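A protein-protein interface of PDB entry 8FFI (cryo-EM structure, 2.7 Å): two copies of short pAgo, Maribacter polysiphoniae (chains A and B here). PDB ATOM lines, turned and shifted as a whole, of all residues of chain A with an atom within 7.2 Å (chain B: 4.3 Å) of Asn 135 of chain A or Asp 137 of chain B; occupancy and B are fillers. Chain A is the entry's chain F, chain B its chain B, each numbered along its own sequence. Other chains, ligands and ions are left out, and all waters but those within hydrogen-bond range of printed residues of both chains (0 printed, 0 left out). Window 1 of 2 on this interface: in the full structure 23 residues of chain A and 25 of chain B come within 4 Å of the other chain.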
ATOM      1  N   TYR A  37      10.784 -15.038 -28.233  1.00  0.00           N
ATOM      2  CA  TYR A  37      12.211 -15.314 -28.224  1.00  0.00           C
ATOM      3  C   TYR A  37      12.839 -15.179 -26.848  1.00  0.00           C
ATOM      4  O   TYR A  37      13.944 -15.691 -26.643  1.00  0.00           O
ATOM      5  CB  TYR A  37      12.943 -14.387 -29.206  1.00  0.00           C
ATOM      6  CG  TYR A  37      12.511 -14.578 -30.641  1.00  0.00           C
ATOM      7  CD1 TYR A  37      12.791 -15.756 -31.319  1.00  0.00           C
ATOM      8  CD2 TYR A  37      11.805 -13.587 -31.311  1.00  0.00           C
ATOM      9  CE1 TYR A  37      12.389 -15.939 -32.628  1.00  0.00           C
ATOM     10  CE2 TYR A  37      11.397 -13.762 -32.618  1.00  0.00           C
ATOM     11  CZ  TYR A  37      11.695 -14.939 -33.272  1.00  0.00           C
ATOM     12  OH  TYR A  37      11.290 -15.113 -34.573  1.00  0.00           O
ATOM     13  N   LYS A  40      12.741  -9.798 -21.702  1.00  0.00           N
ATOM     14  CA  LYS A  40      13.611  -8.854 -21.017  1.00  0.00           C
ATOM     15  C   LYS A  40      12.807  -8.155 -19.931  1.00  0.00           C
ATOM     16  O   LYS A  40      11.701  -7.669 -20.185  1.00  0.00           O
ATOM     17  CB  LYS A  40      14.191  -7.836 -21.998  1.00  0.00           C
ATOM     18  CG  LYS A  40      15.251  -8.404 -22.925  1.00  0.00           C
ATOM     19  CD  LYS A  40      15.652  -7.393 -23.985  1.00  0.00           C
ATOM     20  CE  LYS A  40      14.685  -7.404 -25.155  1.00  0.00           C
ATOM     21  NZ  LYS A  40      15.092  -8.376 -26.206  1.00  0.00           N
ATOM     22  N   SER A  41      13.363  -8.101 -18.725  1.00  0.00           N
ATOM     23  CA  SER A  41      12.625  -7.656 -17.555  1.00  0.00           C
ATOM     24  C   SER A  41      13.231  -6.383 -16.982  1.00  0.00           C
ATOM     25  O   SER A  41      14.437  -6.147 -17.081  1.00  0.00           O
ATOM     26  CB  SER A  41      12.599  -8.742 -16.475  1.00  0.00           C
ATOM     27  OG  SER A  41      13.909  -9.106 -16.085  1.00  0.00           O
ATOM     28  N   GLY A  42      12.373  -5.562 -16.390  1.00  0.00           N
ATOM     29  CA  GLY A  42      12.794  -4.420 -15.594  1.00  0.00           C
ATOM     30  C   GLY A  42      12.335  -4.608 -14.159  1.00  0.00           C
ATOM     31  O   GLY A  42      11.221  -5.081 -13.915  1.00  0.00           O
ATOM     32  N   GLY A  90      18.695 -10.288 -18.655  1.00  0.00           N
ATOM     33  CA  GLY A  90      18.004  -9.193 -19.299  1.00  0.00           C
ATOM     34  C   GLY A  90      17.221  -8.367 -18.303  1.00  0.00           C
ATOM     35  O   GLY A  90      16.088  -7.958 -18.576  1.00  0.00           O
ATOM     36  N   THR A  92      17.089  -4.909 -15.702  1.00  0.00           N
ATOM     37  CA  THR A  92      17.556  -3.519 -15.667  1.00  0.00           C
ATOM     38  C   THR A  92      17.072  -2.913 -14.352  1.00  0.00           C
ATOM     39  O   THR A  92      15.963  -2.381 -14.271  1.00  0.00           O
ATOM     40  CB  THR A  92      17.054  -2.729 -16.868  1.00  0.00           C
ATOM     41  OG1 THR A  92      17.210  -3.512 -18.059  1.00  0.00           O
ATOM     42  CG2 THR A  92      17.841  -1.435 -17.016  1.00  0.00           C
ATOM     43  N   GLU A 132      15.346   6.490 -22.635  1.00  0.00           N
ATOM     44  CA  GLU A 132      16.423   5.514 -22.700  1.00  0.00           C
ATOM     45  C   GLU A 132      16.190   4.549 -23.852  1.00  0.00           C
ATOM     46  O   GLU A 132      15.049   4.266 -24.227  1.00  0.00           O
ATOM     47  CB  GLU A 132      16.563   4.750 -21.376  1.00  0.00           C
ATOM     48  CG  GLU A 132      17.101   5.609 -20.241  1.00  0.00           C
ATOM     49  CD  GLU A 132      17.514   4.798 -19.036  1.00  0.00           C
ATOM     50  OE1 GLU A 132      17.540   3.555 -19.134  1.00  0.00           O
ATOM     51  OE2 GLU A 132      17.817   5.405 -17.990  1.00  0.00           O
ATOM     52  N   ASP A 133      17.293   4.053 -24.414  1.00  0.00           N
ATOM     53  CA  ASP A 133      17.243   3.125 -25.535  1.00  0.00           C
ATOM     54  C   ASP A 133      17.009   1.684 -25.109  1.00  0.00           C
ATOM     55  O   ASP A 133      16.836   0.821 -25.977  1.00  0.00           O
ATOM     56  CB  ASP A 133      18.542   3.206 -26.342  1.00  0.00           C
ATOM     57  CG  ASP A 133      18.705   4.533 -27.054  1.00  0.00           C
ATOM     58  OD1 ASP A 133      17.688   5.094 -27.511  1.00  0.00           O
ATOM     59  OD2 ASP A 133      19.852   5.015 -27.155  1.00  0.00           O
ATOM     60  N   GLU A 134      17.002   1.402 -23.809  1.00  0.00           N
ATOM     61  CA  GLU A 134      16.781   0.041 -23.345  1.00  0.00           C
ATOM     62  C   GLU A 134      15.344  -0.385 -23.618  1.00  0.00           C
ATOM     63  O   GLU A 134      14.403   0.396 -23.451  1.00  0.00           O
ATOM     64  CB  GLU A 134      17.083  -0.074 -21.851  1.00  0.00           C
ATOM     65  CG  GLU A 134      18.529   0.212 -21.478  1.00  0.00           C
ATOM     66  CD  GLU A 134      19.423  -1.006 -21.608  1.00  0.00           C
ATOM     67  OE1 GLU A 134      18.923  -2.137 -21.445  1.00  0.00           O
ATOM     68  OE2 GLU A 134      20.630  -0.828 -21.869  1.00  0.00           O
ATOM     69  N   ASN A 135      15.181  -1.634 -24.039  1.00  0.00           N
ATOM     70  CA  ASN A 135      13.872  -2.204 -24.321  1.00  0.00           C
ATOM     71  C   ASN A 135      13.527  -3.195 -23.215  1.00  0.00           C
ATOM     72  O   ASN A 135      14.182  -4.233 -23.080  1.00  0.00           O
ATOM     73  CB  ASN A 135      13.864  -2.886 -25.690  1.00  0.00           C
ATOM     74  CG  ASN A 135      12.467  -3.245 -26.158  1.00  0.00           C
ATOM     75  OD1 ASN A 135      11.483  -3.012 -25.456  1.00  0.00           O
ATOM     76  ND2 ASN A 135      12.374  -3.815 -27.354  1.00  0.00           N
ATOM     77  N   VAL A 136      12.508  -2.868 -22.424  1.00  0.00           N
ATOM     78  CA  VAL A 136      12.052  -3.713 -21.327  1.00  0.00           C
ATOM     79  C   VAL A 136      10.564  -3.971 -21.514  1.00  0.00           C
ATOM     80  O   VAL A 136       9.793  -3.039 -21.771  1.00  0.00           O
ATOM     81  CB  VAL A 136      12.340  -3.079 -19.951  1.00  0.00           C
ATOM     82  CG1 VAL A 136      13.830  -3.125 -19.653  1.00  0.00           C
ATOM     83  CG2 VAL A 136      11.849  -1.642 -19.909  1.00  0.00           C
ATOM     84  N   ASP A 137      10.163  -5.236 -21.399  1.00  0.00           N
ATOM     85  CA  ASP A 137       8.802  -5.642 -21.739  1.00  0.00           C
ATOM     86  C   ASP A 137       7.869  -5.572 -20.533  1.00  0.00           C
ATOM     87  O   ASP A 137       6.872  -4.842 -20.553  1.00  0.00           O
ATOM     88  CB  ASP A 137       8.818  -7.056 -22.330  1.00  0.00           C
ATOM     89  CG  ASP A 137       9.771  -7.182 -23.498  1.00  0.00           C
ATOM     90  OD1 ASP A 137       9.989  -6.173 -24.198  1.00  0.00           O
ATOM     91  OD2 ASP A 137      10.307  -8.289 -23.710  1.00  0.00           O
ATOM     92  N   GLY B  38      15.530 -11.840 -30.239  1.00  0.00           N
ATOM     93  CA  GLY B  38      14.893 -11.881 -31.537  1.00  0.00           C
ATOM     94  C   GLY B  38      14.024 -10.667 -31.774  1.00  0.00           C
ATOM     95  O   GLY B  38      13.441 -10.121 -30.834  1.00  0.00           O
ATOM     96  N   ILE B  39      13.926 -10.233 -33.025  1.00  0.00           N
ATOM     97  CA  ILE B  39      13.166  -9.043 -33.384  1.00  0.00           C
ATOM     98  C   ILE B  39      11.793  -9.478 -33.874  1.00  0.00           C
ATOM     99  O   ILE B  39      11.681 -10.201 -34.872  1.00  0.00           O
ATOM    100  CB  ILE B  39      13.896  -8.213 -34.452  1.00  0.00           C
ATOM    101  CG1 ILE B  39      15.170  -7.594 -33.873  1.00  0.00           C
ATOM    102  CG2 ILE B  39      12.982  -7.131 -34.999  1.00  0.00           C
ATOM    103  CD1 ILE B  39      16.162  -7.146 -34.920  1.00  0.00           C
ATOM    104  N   LYS B  40      10.750  -9.047 -33.171  1.00  0.00           N
ATOM    105  CA  LYS B  40       9.372  -9.230 -33.607  1.00  0.00           C
ATOM    106  C   LYS B  40       8.909  -7.930 -34.247  1.00  0.00           C
ATOM    107  O   LYS B  40       8.863  -6.890 -33.583  1.00  0.00           O
ATOM    108  CB  LYS B  40       8.468  -9.614 -32.437  1.00  0.00           C
ATOM    109  CG  LYS B  40       8.574 -11.072 -32.015  1.00  0.00           C
ATOM    110  CD  LYS B  40       7.713 -11.354 -30.796  1.00  0.00           C
ATOM    111  CE  LYS B  40       8.317 -10.746 -29.542  1.00  0.00           C
ATOM    112  NZ  LYS B  40       9.058 -11.755 -28.734  1.00  0.00           N
ATOM    113  N   VAL B 136       5.365  -5.892 -30.414  1.00  0.00           N
ATOM    114  CA  VAL B 136       6.120  -5.466 -31.585  1.00  0.00           C
ATOM    115  C   VAL B 136       7.304  -4.637 -31.113  1.00  0.00           C
ATOM    116  O   VAL B 136       7.149  -3.745 -30.271  1.00  0.00           O
ATOM    117  CB  VAL B 136       5.237  -4.666 -32.562  1.00  0.00           C
ATOM    118  CG1 VAL B 136       6.090  -3.926 -33.570  1.00  0.00           C
ATOM    119  CG2 VAL B 136       4.255  -5.588 -33.263  1.00  0.00           C
ATOM    120  N   ASP B 137       8.488  -4.938 -31.647  1.00  0.00           N
ATOM    121  CA  ASP B 137       9.687  -4.180 -31.312  1.00  0.00           C
ATOM    122  C   ASP B 137       9.866  -2.965 -32.214  1.00  0.00           C
ATOM    123  O   ASP B 137      10.096  -1.856 -31.720  1.00  0.00           O
ATOM    124  CB  ASP B 137      10.922  -5.079 -31.398  1.00  0.00           C
ATOM    125  CG  ASP B 137      10.770  -6.356 -30.595  1.00  0.00           C
ATOM    126  OD1 ASP B 137      10.431  -6.272 -29.395  1.00  0.00           O
ATOM    127  OD2 ASP B 137      10.990  -7.446 -31.162  1.00  0.00           O
ATOM    128  N   VAL B 138       9.763  -3.153 -33.529  1.00  0.00           N
ATOM    129  CA  VAL B 138       9.878  -2.068 -34.494  1.00  0.00           C
ATOM    130  C   VAL B 138       8.724  -2.176 -35.480  1.00  0.00           C
ATOM    131  O   VAL B 138       8.314  -3.274 -35.866  1.00  0.00           O
ATOM    132  CB  VAL B 138      11.233  -2.093 -35.246  1.00  0.00           C
ATOM    133  CG1 VAL B 138      11.445  -0.798 -36.012  1.00  0.00           C
ATOM    134  CG2 VAL B 138      12.387  -2.337 -34.286  1.00  0.00           C
ATOM    135  N   PRO B 220       8.991   2.943 -31.660  1.00  0.00           N
ATOM    136  CA  PRO B 220      10.081   2.910 -32.642  1.00  0.00           C
ATOM    137  C   PRO B 220       9.568   2.447 -33.995  1.00  0.00           C
ATOM    138  O   PRO B 220       8.854   1.448 -34.100  1.00  0.00           O
ATOM    139  CB  PRO B 220      11.074   1.909 -32.041  1.00  0.00           C
ATOM    140  CG  PRO B 220      10.725   1.842 -30.589  1.00  0.00           C
ATOM    141  CD  PRO B 220       9.249   2.057 -30.514  1.00  0.00           C
ATOM    142  N   ALA B 264      15.711  -1.710 -32.190  1.00  0.00           N
ATOM    143  CA  ALA B 264      15.041  -2.710 -31.370  1.00  0.00           C
ATOM    144  C   ALA B 264      15.684  -2.872 -29.999  1.00  0.00           C
ATOM    145  O   ALA B 264      15.363  -3.827 -29.287  1.00  0.00           O
ATOM    146  CB  ALA B 264      15.015  -4.054 -32.096  1.00  0.00           C
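Printed residues of chain A that touch a printed residue of chain B: Tyr 37 and Asn 135. Hydrophobic or aromatic side chains of chain A that line the printed part of chain B: Tyr 37. Along chain A the printed residues that touch a printed residue of chain B span positions 37 to 135. Among the printed residues, no Asp or Glu carboxylate lies within 4 Å of a Lys or Arg side-chain nitrogen of the other chain.
The backbone NH of Lys 40 of chain B sits at hydrogen-bond distance from the side-chain carboxylate of Asp 137 of chain B (2.6 Å).
Of the printed residues of chain A, Asp 137 of chain B touches Asn 135. Of the printed residues of chain B, Tyr 37 of chain A touches Gly 38 and Lys 40. Printed residues of chain A within 4 Å of Ala 264 of chain B: Asn 135. Val 136 of chain A touches none of the printed residues of chain B. The nearest printed residue of chain B that does not touch Tyr 37 of chain A is Ile 39 of chain B (4.2 Å).
Positions printed for both chains: 40, 136 and 137.
Among the printed residues, merely in contact across the chains: Tyr 37 of chain A with Gly 38 of chain B (3.5 Å), Asn 135 of chain A with Ala 264 of chain B (3.6 Å), Asn 135 of chain A with Asp 137 of chain B (3.7 Å) and Tyr 37 of chain A with Lys 40 of chain B (3.7 Å).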
